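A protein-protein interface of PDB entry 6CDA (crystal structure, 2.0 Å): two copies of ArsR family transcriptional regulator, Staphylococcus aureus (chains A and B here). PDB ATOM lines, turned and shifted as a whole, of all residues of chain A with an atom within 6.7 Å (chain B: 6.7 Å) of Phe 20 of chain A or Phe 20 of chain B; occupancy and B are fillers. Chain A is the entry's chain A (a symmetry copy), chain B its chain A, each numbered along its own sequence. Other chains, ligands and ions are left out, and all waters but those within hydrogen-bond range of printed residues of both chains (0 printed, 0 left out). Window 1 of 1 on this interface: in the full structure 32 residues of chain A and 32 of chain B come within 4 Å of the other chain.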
ATOM      1  N   ARG A  15      -4.905  27.494 -10.412  1.00  0.00           N
ATOM      2  CA  ARG A  15      -4.354  26.700  -9.317  1.00  0.00           C
ATOM      3  C   ARG A  15      -4.758  25.246  -9.468  1.00  0.00           C
ATOM      4  O   ARG A  15      -3.979  24.342  -9.151  1.00  0.00           O
ATOM      5  CB  ARG A  15      -4.829  27.236  -7.964  1.00  0.00           C
ATOM      6  CG  ARG A  15      -4.171  28.554  -7.548  1.00  0.00           C
ATOM      7  CD  ARG A  15      -4.721  29.149  -6.223  1.00  0.00           C
ATOM      8  NE  ARG A  15      -6.101  29.638  -6.353  1.00  0.00           N
ATOM      9  CZ  ARG A  15      -6.684  30.558  -5.575  1.00  0.00           C
ATOM     10  NH1 ARG A  15      -6.013  31.133  -4.576  1.00  0.00           N
ATOM     11  NH2 ARG A  15      -7.954  30.913  -5.802  1.00  0.00           N
ATOM     12  N   VAL A  16      -5.974  25.005  -9.958  1.00  0.00           N
ATOM     13  CA  VAL A  16      -6.429  23.642 -10.185  1.00  0.00           C
ATOM     14  C   VAL A  16      -5.585  22.986 -11.271  1.00  0.00           C
ATOM     15  O   VAL A  16      -5.254  21.798 -11.183  1.00  0.00           O
ATOM     16  CB  VAL A  16      -7.928  23.615 -10.540  1.00  0.00           C
ATOM     17  CG1 VAL A  16      -8.315  22.251 -11.011  1.00  0.00           C
ATOM     18  CG2 VAL A  16      -8.815  23.940  -9.334  1.00  0.00           C
ATOM     19  N   THR A  17      -5.222  23.728 -12.318  1.00  0.00           N
ATOM     20  CA  THR A  17      -4.446  23.072 -13.365  1.00  0.00           C
ATOM     21  C   THR A  17      -3.031  22.775 -12.886  1.00  0.00           C
ATOM     22  O   THR A  17      -2.465  21.743 -13.251  1.00  0.00           O
ATOM     23  CB  THR A  17      -4.422  23.886 -14.656  1.00  0.00           C
ATOM     24  OG1 THR A  17      -3.780  25.138 -14.437  1.00  0.00           O
ATOM     25  CG2 THR A  17      -5.808  24.112 -15.131  1.00  0.00           C
ATOM     26  N   GLU A  18      -2.443  23.636 -12.049  1.00  0.00           N
ATOM     27  CA  GLU A  18      -1.103  23.303 -11.558  1.00  0.00           C
ATOM     28  C   GLU A  18      -1.150  22.106 -10.610  1.00  0.00           C
ATOM     29  O   GLU A  18      -0.186  21.337 -10.542  1.00  0.00           O
ATOM     30  CB  GLU A  18      -0.444  24.515 -10.888  1.00  0.00           C
ATOM     31  CG  GLU A  18      -0.190  25.774 -11.820  1.00  0.00           C
ATOM     32  CD  GLU A  18       0.530  25.512 -13.195  1.00  0.00           C
ATOM     33  OE1 GLU A  18      -0.150  25.543 -14.263  1.00  0.00           O
ATOM     34  OE2 GLU A  18       1.779  25.333 -13.216  1.00  0.00           O
ATOM     35  N   ILE A  19      -2.262  21.928  -9.877  1.00  0.00           N
ATOM     36  CA  ILE A  19      -2.443  20.740  -9.035  1.00  0.00           C
ATOM     37  C   ILE A  19      -2.440  19.486  -9.892  1.00  0.00           C
ATOM     38  O   ILE A  19      -1.707  18.525  -9.634  1.00  0.00           O
ATOM     39  CB  ILE A  19      -3.747  20.848  -8.214  1.00  0.00           C
ATOM     40  CG1 ILE A  19      -3.567  21.793  -7.010  1.00  0.00           C
ATOM     41  CG2 ILE A  19      -4.199  19.478  -7.743  1.00  0.00           C
ATOM     42  CD1 ILE A  19      -4.876  22.186  -6.299  1.00  0.00           C
ATOM     43  N   PHE A  20      -3.299  19.457 -10.903  1.00  0.00           N
ATOM     44  CA  PHE A  20      -3.377  18.274 -11.740  1.00  0.00           C
ATOM     45  C   PHE A  20      -2.089  18.099 -12.526  1.00  0.00           C
ATOM     46  O   PHE A  20      -1.581  16.976 -12.650  1.00  0.00           O
ATOM     47  CB  PHE A  20      -4.616  18.368 -12.657  1.00  0.00           C
ATOM     48  CG  PHE A  20      -5.929  18.193 -11.925  1.00  0.00           C
ATOM     49  CD1 PHE A  20      -6.979  19.053 -12.144  1.00  0.00           C
ATOM     50  CD2 PHE A  20      -6.123  17.142 -11.064  1.00  0.00           C
ATOM     51  CE1 PHE A  20      -8.167  18.875 -11.487  1.00  0.00           C
ATOM     52  CE2 PHE A  20      -7.307  16.983 -10.395  1.00  0.00           C
ATOM     53  CZ  PHE A  20      -8.324  17.831 -10.612  1.00  0.00           C
ATOM     54  N   LYS A  21      -1.533  19.197 -13.046  1.00  0.00           N
ATOM     55  CA  LYS A  21      -0.217  19.141 -13.679  1.00  0.00           C
ATOM     56  C   LYS A  21       0.780  18.461 -12.774  1.00  0.00           C
ATOM     57  O   LYS A  21       1.562  17.615 -13.215  1.00  0.00           O
ATOM     58  CB  LYS A  21       0.296  20.545 -14.008  1.00  0.00           C
ATOM     59  CG  LYS A  21       0.480  20.826 -15.462  1.00  0.00           C
ATOM     60  CD  LYS A  21       0.640  22.344 -15.693  1.00  0.00           C
ATOM     61  CE  LYS A  21       0.481  22.744 -17.165  1.00  0.00           C
ATOM     62  NZ  LYS A  21       0.241  24.212 -17.374  1.00  0.00           N
ATOM     63  N   ALA A  22       0.782  18.841 -11.498  1.00  0.00           N
ATOM     64  CA  ALA A  22       1.756  18.279 -10.584  1.00  0.00           C
ATOM     65  C   ALA A  22       1.527  16.795 -10.416  1.00  0.00           C
ATOM     66  O   ALA A  22       2.482  16.045 -10.205  1.00  0.00           O
ATOM     67  CB  ALA A  22       1.675  18.970  -9.221  1.00  0.00           C
ATOM     68  N   LEU A  23       0.269  16.346 -10.515  1.00  0.00           N
ATOM     69  CA  LEU A  23      -0.042  14.939 -10.309  1.00  0.00           C
ATOM     70  C   LEU A  23       0.176  14.065 -11.533  1.00  0.00           C
ATOM     71  O   LEU A  23       0.063  12.845 -11.423  1.00  0.00           O
ATOM     72  CB  LEU A  23      -1.481  14.794  -9.855  1.00  0.00           C
ATOM     73  CG  LEU A  23      -1.674  15.431  -8.478  1.00  0.00           C
ATOM     74  CD1 LEU A  23      -3.135  15.511  -8.211  1.00  0.00           C
ATOM     75  CD2 LEU A  23      -1.001  14.638  -7.409  1.00  0.00           C
ATOM     76  N   GLY A  24       0.473  14.636 -12.691  1.00  0.00           N
ATOM     77  CA  GLY A  24       0.668  13.840 -13.890  1.00  0.00           C
ATOM     78  C   GLY A  24       2.048  13.256 -14.042  1.00  0.00           C
ATOM     79  O   GLY A  24       2.677  13.419 -15.088  1.00  0.00           O
ATOM     80  N   ASP A  25       2.535  12.575 -13.010  1.00  0.00           N
ATOM     81  CA  ASP A  25       3.900  12.051 -12.997  1.00  0.00           C
ATOM     82  C   ASP A  25       3.898  10.795 -12.145  1.00  0.00           C
ATOM     83  O   ASP A  25       3.375  10.794 -11.024  1.00  0.00           O
ATOM     84  CB  ASP A  25       4.903  13.067 -12.450  1.00  0.00           C
ATOM     85  CG  ASP A  25       6.313  12.505 -12.375  1.00  0.00           C
ATOM     86  OD1 ASP A  25       6.666  11.900 -11.360  1.00  0.00           O
ATOM     87  OD2 ASP A  25       7.072  12.666 -13.335  1.00  0.00           O
ATOM     88  N   ILE A  29       2.861  10.304  -8.148  1.00  0.00           N
ATOM     89  CA  ILE A  29       1.697   9.531  -7.735  1.00  0.00           C
ATOM     90  C   ILE A  29       2.093   8.447  -6.739  1.00  0.00           C
ATOM     91  O   ILE A  29       1.352   8.181  -5.785  1.00  0.00           O
ATOM     92  CB  ILE A  29       0.984   8.939  -8.957  1.00  0.00           C
ATOM     93  CG1 ILE A  29       0.337  10.051  -9.798  1.00  0.00           C
ATOM     94  CG2 ILE A  29      -0.073   7.920  -8.501  1.00  0.00           C
ATOM     95  CD1 ILE A  29      -0.609  10.918  -9.033  1.00  0.00           C
ATOM     96  N   LEU A  68      -0.150  20.151  -2.148  1.00  0.00           N
ATOM     97  CA  LEU A  68      -0.630  18.785  -2.095  1.00  0.00           C
ATOM     98  C   LEU A  68      -0.055  18.038  -0.910  1.00  0.00           C
ATOM     99  O   LEU A  68      -0.719  17.144  -0.400  1.00  0.00           O
ATOM    100  CB  LEU A  68      -0.290  18.062  -3.396  1.00  0.00           C
ATOM    101  CG  LEU A  68      -1.130  18.552  -4.572  1.00  0.00           C
ATOM    102  CD1 LEU A  68      -0.574  17.976  -5.831  1.00  0.00           C
ATOM    103  CD2 LEU A  68      -2.530  18.100  -4.377  1.00  0.00           C
ATOM    104  N   MET A  90      -9.479  13.364  -3.205  1.00  0.00           N
ATOM    105  CA  MET A  90      -9.180  13.479  -4.622  1.00  0.00           C
ATOM    106  C   MET A  90      -8.362  12.292  -5.113  1.00  0.00           C
ATOM    107  O   MET A  90      -8.696  11.665  -6.128  1.00  0.00           O
ATOM    108  CB  MET A  90      -8.461  14.805  -4.841  1.00  0.00           C
ATOM    109  CG  MET A  90      -8.248  15.218  -6.252  1.00  0.00           C
ATOM    110  SD  MET A  90      -7.144  16.666  -6.365  1.00  0.00           S
ATOM    111  CE  MET A  90      -5.606  15.851  -6.326  1.00  0.00           C
ATOM    112  N   LEU A  91      -7.292  11.954  -4.401  1.00  0.00           N
ATOM    113  CA  LEU A  91      -6.449  10.841  -4.824  1.00  0.00           C
ATOM    114  C   LEU A  91      -7.212   9.522  -4.746  1.00  0.00           C
ATOM    115  O   LEU A  91      -7.164   8.702  -5.669  1.00  0.00           O
ATOM    116  CB  LEU A  91      -5.171  10.790  -3.958  1.00  0.00           C
ATOM    117  CG  LEU A  91      -4.067   9.766  -4.306  1.00  0.00           C
ATOM    118  CD1 LEU A  91      -3.456  10.054  -5.684  1.00  0.00           C
ATOM    119  CD2 LEU A  91      -2.931   9.671  -3.229  1.00  0.00           C
ATOM    120  N   ALA A  94      -9.712   9.114  -7.554  1.00  0.00           N
ATOM    121  CA  ALA A  94      -8.995   8.825  -8.790  1.00  0.00           C
ATOM    122  C   ALA A  94      -8.596   7.355  -8.883  1.00  0.00           C
ATOM    123  O   ALA A  94      -8.784   6.700  -9.924  1.00  0.00           O
ATOM    124  CB  ALA A  94      -7.773   9.736  -8.862  1.00  0.00           C
ATOM    125  N   ILE A  95      -8.065   6.803  -7.790  1.00  0.00           N
ATOM    126  CA  ILE A  95      -7.647   5.405  -7.794  1.00  0.00           C
ATOM    127  C   ILE A  95      -8.854   4.471  -7.881  1.00  0.00           C
ATOM    128  O   ILE A  95      -8.853   3.499  -8.649  1.00  0.00           O
ATOM    129  CB  ILE A  95      -6.767   5.126  -6.560  1.00  0.00           C
ATOM    130  CG1 ILE A  95      -5.500   5.959  -6.668  1.00  0.00           C
ATOM    131  CG2 ILE A  95      -6.367   3.668  -6.502  1.00  0.00           C
ATOM    132  CD1 ILE A  95      -4.649   5.945  -5.381  1.00  0.00           C
ATOM    133  N   ARG B  15      -2.802   4.380 -15.174  1.00  0.00           N
ATOM    134  CA  ARG B  15      -4.083   4.964 -15.567  1.00  0.00           C
ATOM    135  C   ARG B  15      -4.354   6.222 -14.766  1.00  0.00           C
ATOM    136  O   ARG B  15      -4.921   7.187 -15.286  1.00  0.00           O
ATOM    137  CB  ARG B  15      -5.221   3.961 -15.366  1.00  0.00           C
ATOM    138  CG  ARG B  15      -5.243   2.826 -16.394  1.00  0.00           C
ATOM    139  CD  ARG B  15      -6.338   1.755 -16.135  1.00  0.00           C
ATOM    140  NE  ARG B  15      -6.065   0.946 -14.939  1.00  0.00           N
ATOM    141  CZ  ARG B  15      -6.542  -0.281 -14.696  1.00  0.00           C
ATOM    142  NH1 ARG B  15      -7.337  -0.892 -15.575  1.00  0.00           N
ATOM    143  NH2 ARG B  15      -6.216  -0.909 -13.561  1.00  0.00           N
ATOM    144  N   VAL B  16      -3.947   6.229 -13.496  1.00  0.00           N
ATOM    145  CA  VAL B  16      -4.120   7.410 -12.665  1.00  0.00           C
ATOM    146  C   VAL B  16      -3.273   8.555 -13.207  1.00  0.00           C
ATOM    147  O   VAL B  16      -3.701   9.715 -13.202  1.00  0.00           O
ATOM    148  CB  VAL B  16      -3.779   7.101 -11.194  1.00  0.00           C
ATOM    149  CG1 VAL B  16      -3.718   8.372 -10.409  1.00  0.00           C
ATOM    150  CG2 VAL B  16      -4.835   6.214 -10.529  1.00  0.00           C
ATOM    151  N   THR B  17      -2.059   8.270 -13.679  1.00  0.00           N
ATOM    152  CA  THR B  17      -1.249   9.385 -14.159  1.00  0.00           C
ATOM    153  C   THR B  17      -1.801   9.931 -15.469  1.00  0.00           C
ATOM    154  O   THR B  17      -1.751  11.141 -15.697  1.00  0.00           O
ATOM    155  CB  THR B  17       0.222   9.003 -14.307  1.00  0.00           C
ATOM    156  OG1 THR B  17       0.368   7.980 -15.287  1.00  0.00           O
ATOM    157  CG2 THR B  17       0.749   8.528 -13.005  1.00  0.00           C
ATOM    158  N   GLU B  18      -2.359   9.080 -16.336  1.00  0.00           N
ATOM    159  CA  GLU B  18      -2.932   9.635 -17.565  1.00  0.00           C
ATOM    160  C   GLU B  18      -4.184  10.455 -17.262  1.00  0.00           C
ATOM    161  O   GLU B  18      -4.476  11.419 -17.977  1.00  0.00           O
ATOM    162  CB  GLU B  18      -3.229   8.527 -18.584  1.00  0.00           C
ATOM    163  CG  GLU B  18      -1.975   7.704 -19.104  1.00  0.00           C
ATOM    164  CD  GLU B  18      -0.737   8.533 -19.614  1.00  0.00           C
ATOM    165  OE1 GLU B  18       0.298   8.604 -18.888  1.00  0.00           O
ATOM    166  OE2 GLU B  18      -0.776   9.062 -20.759  1.00  0.00           O
ATOM    167  N   ILE B  19      -4.931  10.096 -16.204  1.00  0.00           N
ATOM    168  CA  ILE B  19      -6.078  10.899 -15.767  1.00  0.00           C
ATOM    169  C   ILE B  19      -5.618  12.287 -15.356  1.00  0.00           C
ATOM    170  O   ILE B  19      -6.146  13.307 -15.812  1.00  0.00           O
ATOM    171  CB  ILE B  19      -6.826  10.197 -14.612  1.00  0.00           C
ATOM    172  CG1 ILE B  19      -7.708   9.049 -15.140  1.00  0.00           C
ATOM    173  CG2 ILE B  19      -7.669  11.192 -13.836  1.00  0.00           C
ATOM    174  CD1 ILE B  19      -8.269   8.115 -14.050  1.00  0.00           C
ATOM    175  N   PHE B  20      -4.654  12.346 -14.446  1.00  0.00           N
ATOM    176  CA  PHE B  20      -4.192  13.640 -13.980  1.00  0.00           C
ATOM    177  C   PHE B  20      -3.497  14.389 -15.103  1.00  0.00           C
ATOM    178  O   PHE B  20      -3.704  15.599 -15.268  1.00  0.00           O
ATOM    179  CB  PHE B  20      -3.280  13.452 -12.747  1.00  0.00           C
ATOM    180  CG  PHE B  20      -4.024  13.032 -11.498  1.00  0.00           C
ATOM    181  CD1 PHE B  20      -3.561  12.001 -10.714  1.00  0.00           C
ATOM    182  CD2 PHE B  20      -5.150  13.701 -11.088  1.00  0.00           C
ATOM    183  CE1 PHE B  20      -4.235  11.641  -9.578  1.00  0.00           C
ATOM    184  CE2 PHE B  20      -5.830  13.320  -9.962  1.00  0.00           C
ATOM    185  CZ  PHE B  20      -5.373  12.310  -9.207  1.00  0.00           C
ATOM    186  N   LYS B  21      -2.686  13.687 -15.899  1.00  0.00           N
ATOM    187  CA  LYS B  21      -2.103  14.292 -17.095  1.00  0.00           C
ATOM    188  C   LYS B  21      -3.171  14.952 -17.932  1.00  0.00           C
ATOM    189  O   LYS B  21      -2.997  16.075 -18.412  1.00  0.00           O
ATOM    190  CB  LYS B  21      -1.388  13.244 -17.950  1.00  0.00           C
ATOM    191  CG  LYS B  21       0.085  13.443 -18.091  1.00  0.00           C
ATOM    192  CD  LYS B  21       0.742  12.161 -18.647  1.00  0.00           C
ATOM    193  CE  LYS B  21       2.268  12.156 -18.491  1.00  0.00           C
ATOM    194  NZ  LYS B  21       2.892  10.800 -18.652  1.00  0.00           N
ATOM    195  N   ALA B  22      -4.285  14.251 -18.138  1.00  0.00           N
ATOM    196  CA  ALA B  22      -5.327  14.792 -18.986  1.00  0.00           C
ATOM    197  C   ALA B  22      -5.914  16.041 -18.368  1.00  0.00           C
ATOM    198  O   ALA B  22      -6.336  16.945 -19.091  1.00  0.00           O
ATOM    199  CB  ALA B  22      -6.433  13.758 -19.206  1.00  0.00           C
ATOM    200  N   LEU B  23      -5.941  16.118 -17.032  1.00  0.00           N
ATOM    201  CA  LEU B  23      -6.541  17.261 -16.359  1.00  0.00           C
ATOM    202  C   LEU B  23      -5.622  18.464 -16.231  1.00  0.00           C
ATOM    203  O   LEU B  23      -6.078  19.519 -15.794  1.00  0.00           O
ATOM    204  CB  LEU B  23      -7.010  16.853 -14.976  1.00  0.00           C
ATOM    205  CG  LEU B  23      -8.144  15.832 -15.075  1.00  0.00           C
ATOM    206  CD1 LEU B  23      -8.369  15.265 -13.719  1.00  0.00           C
ATOM    207  CD2 LEU B  23      -9.400  16.456 -15.584  1.00  0.00           C
ATOM    208  N   GLY B  24      -4.350  18.347 -16.584  1.00  0.00           N
ATOM    209  CA  GLY B  24      -3.432  19.465 -16.457  1.00  0.00           C
ATOM    210  C   GLY B  24      -3.463  20.439 -17.605  1.00  0.00           C
ATOM    211  O   GLY B  24      -2.417  20.761 -18.171  1.00  0.00           O
ATOM    212  N   ASP B  25      -4.649  20.918 -17.962  1.00  0.00           N
ATOM    213  CA  ASP B  25      -4.820  21.787 -19.126  1.00  0.00           C
ATOM    214  C   ASP B  25      -5.997  22.703 -18.842  1.00  0.00           C
ATOM    215  O   ASP B  25      -7.068  22.242 -18.427  1.00  0.00           O
ATOM    216  CB  ASP B  25      -5.057  20.994 -20.410  1.00  0.00           C
ATOM    217  CG  ASP B  25      -5.298  21.894 -21.611  1.00  0.00           C
ATOM    218  OD1 ASP B  25      -6.447  22.268 -21.860  1.00  0.00           O
ATOM    219  OD2 ASP B  25      -4.337  22.231 -22.308  1.00  0.00           O
ATOM    220  N   ILE B  29      -9.961  21.746 -18.023  1.00  0.00           N
ATOM    221  CA  ILE B  29     -10.572  22.005 -16.726  1.00  0.00           C
ATOM    222  C   ILE B  29     -11.840  22.837 -16.883  1.00  0.00           C
ATOM    223  O   ILE B  29     -12.827  22.602 -16.173  1.00  0.00           O
ATOM    224  CB  ILE B  29      -9.568  22.681 -15.784  1.00  0.00           C
ATOM    225  CG1 ILE B  29      -8.440  21.709 -15.408  1.00  0.00           C
ATOM    226  CG2 ILE B  29     -10.292  23.185 -14.525  1.00  0.00           C
ATOM    227  CD1 ILE B  29      -8.918  20.430 -14.802  1.00  0.00           C
ATOM    228  N   LEU B  68     -12.856  10.190 -18.335  1.00  0.00           N
ATOM    229  CA  LEU B  68     -13.297  11.289 -17.501  1.00  0.00           C
ATOM    230  C   LEU B  68     -14.651  11.811 -17.936  1.00  0.00           C
ATOM    231  O   LEU B  68     -15.392  12.299 -17.093  1.00  0.00           O
ATOM    232  CB  LEU B  68     -12.261  12.410 -17.525  1.00  0.00           C
ATOM    233  CG  LEU B  68     -10.989  12.045 -16.765  1.00  0.00           C
ATOM    234  CD1 LEU B  68      -9.952  13.082 -17.040  1.00  0.00           C
ATOM    235  CD2 LEU B  68     -11.299  12.002 -15.315  1.00  0.00           C
ATOM    236  N   MET B  90     -13.745  14.019  -7.438  1.00  0.00           N
ATOM    237  CA  MET B  90     -12.356  14.393  -7.645  1.00  0.00           C
ATOM    238  C   MET B  90     -12.232  15.852  -8.062  1.00  0.00           C
ATOM    239  O   MET B  90     -11.439  16.613  -7.489  1.00  0.00           O
ATOM    240  CB  MET B  90     -11.769  13.445  -8.685  1.00  0.00           C
ATOM    241  CG  MET B  90     -10.300  13.519  -8.894  1.00  0.00           C
ATOM    242  SD  MET B  90      -9.782  12.540 -10.344  1.00  0.00           S
ATOM    243  CE  MET B  90     -10.062  13.720 -11.593  1.00  0.00           C
ATOM    244  N   LEU B  91     -13.018  16.272  -9.048  1.00  0.00           N
ATOM    245  CA  LEU B  91     -12.938  17.653  -9.514  1.00  0.00           C
ATOM    246  C   LEU B  91     -13.388  18.621  -8.424  1.00  0.00           C
ATOM    247  O   LEU B  91     -12.740  19.642  -8.171  1.00  0.00           O
ATOM    248  CB  LEU B  91     -13.789  17.827 -10.791  1.00  0.00           C
ATOM    249  CG  LEU B  91     -13.756  19.180 -11.538  1.00  0.00           C
ATOM    250  CD1 LEU B  91     -12.357  19.474 -12.096  1.00  0.00           C
ATOM    251  CD2 LEU B  91     -14.822  19.295 -12.683  1.00  0.00           C
ATOM    252  N   ALA B  94     -10.802  19.054  -5.699  1.00  0.00           N
ATOM    253  CA  ALA B  94      -9.706  19.868  -6.209  1.00  0.00           C
ATOM    254  C   ALA B  94     -10.042  21.355  -6.177  1.00  0.00           C
ATOM    255  O   ALA B  94      -9.232  22.190  -5.734  1.00  0.00           O
ATOM    256  CB  ALA B  94      -9.381  19.404  -7.627  1.00  0.00           C
ATOM    257  N   ILE B  95     -11.250  21.712  -6.616  1.00  0.00           N
ATOM    258  CA  ILE B  95     -11.651  23.114  -6.630  1.00  0.00           C
ATOM    259  C   ILE B  95     -11.830  23.647  -5.208  1.00  0.00           C
ATOM    260  O   ILE B  95     -11.374  24.752  -4.880  1.00  0.00           O
ATOM    261  CB  ILE B  95     -12.918  23.282  -7.491  1.00  0.00           C
ATOM    262  CG1 ILE B  95     -12.582  22.912  -8.927  1.00  0.00           C
ATOM    263  CG2 ILE B  95     -13.395  24.717  -7.474  1.00  0.00           C
ATOM    264  CD1 ILE B  95     -13.823  22.814  -9.838  1.00  0.00           C
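OE1 of Glu 18 of chain B lies within salt-bridge range of NZ of Lys 21 of chain B (3.4 Å).
OE1 of Glu 18 of chain A is in salt-bridge range of NZ of Lys 21 of chain A (3.4 Å).
Phe 20 of chain B touches its own counterpart, Phe 20 of chain A.
Phe 20 of chain A touches Ile 29 of chain B, and with the chains exchanged Ile 29 of chain A touches Phe 20 of chain B.
Lys 21 of chain A touches Gly 24 of chain B, and with the chains exchanged Gly 24 of chain A touches Lys 21 of chain B.
Met 90 of chain A touches Ala 94 of chain B, and with the chains exchanged Ala 94 of chain A touches Met 90 of chain B.
Positions printed for both chains: 15, 16, 17, 18, 19, 20, 21, 22, 23, 24, 25, 29, 68, 90, 91, 94 and 95.
Of the 20 pairs that touch across the chains among the printed residues, 20 have their exchanged pair printed and touching as well.
Printed residues of chain B that touch a printed residue of chain A: Val 16, Thr 17, Phe 20, Lys 21, Leu 23, Gly 24, Asp 25, Ile 29, Met 90, Ala 94 and Ile 95.
Hydrophobic or aromatic side chains of chain B that line the printed part of chain A: Val 16, Phe 20, Leu 23, Ile 29, Met 90, Ala 94 and Ile 95.
Among the printed residues, 20 pairs touch across the chains.
Among the printed residues, pairs that only touch across the chains: Val 16 of chain A with Ile 95 of chain B (3.9 Å), Thr 17 of chain A with Asp 25 of chain B (3.97 Å), Thr 17 of chain A with Ile 29 of chain B (3.6 Å), Phe 20 of chain A with Phe 20 of chain B (3.6 Å), Phe 20 of chain A with Leu 23 of chain B (3.5 Å), Phe 20 of chain A with Gly 24 of chain B (3.9 Å), Phe 20 of chain A with Ile 29 of chain B (3.6 Å), Phe 20 of chain A with Ala 94 of chain B (3.5 Å), Lys 21 of chain A with Gly 24 of chain B (3.7 Å), Leu 23 of chain A with Phe 20 of chain B (3.5 Å), Gly 24 of chain A with Phe 20 of chain B (3.9 Å), Gly 24 of chain A with Lys 21 of chain B (3.7 Å), Asp 25 of chain A with Thr 17 of chain B (3.97 Å), Ile 29 of chain A with Thr 17 of chain B (3.6 Å), Ile 29 of chain A with Phe 20 of chain B (3.6 Å), Met 90 of chain A with Met 90 of chain B (3.7 Å), Met 90 of chain A with Ala 94 of chain B (3.8 Å), Ala 94 of chain A with Phe 20 of chain B (3.5 Å), Ala 94 of chain A with Met 90 of chain B (3.8 Å) and Ile 95 of chain A with Val 16 of chain B (3.9 Å).
Of chain B, only Phe 20, Leu 23, Gly 24, Ile 29 and Ala 94 come within 4 Å of Phe 20 of chain A.
Of the printed residues of chain B, Ile 29 of chain A touches Thr 17 (3.6 Å) and Phe 20 (3.6 Å).
Of chain A, only Phe 20, Leu 23, Gly 24, Ile 29 and Ala 94 come within 4 Å of Phe 20 of chain B.
Of the printed residues of chain A, Lys 21 of chain B touches Gly 24 (3.7 Å).
Of the printed residues of chain A, Ile 29 of chain B touches Thr 17 and Phe 20.
Printed residues of chain A within 4 Å of Met 90 of chain B: Met 90 (3.7 Å) and Ala 94 (3.8 Å).
Of the printed residues of chain A, Ala 94 of chain B touches Phe 20 and Met 90.
The nearest residue of chain B that does not touch Phe 20 of chain A is Leu 91 of chain B (4.3 Å).
The nearest residue of chain A that does not touch Phe 20 of chain B is Leu 91 of chain A (4.3 Å).
The nearest printed residue of chain B that does not touch Gly 24 of chain A is Thr 17 of chain B (4.05 Å).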
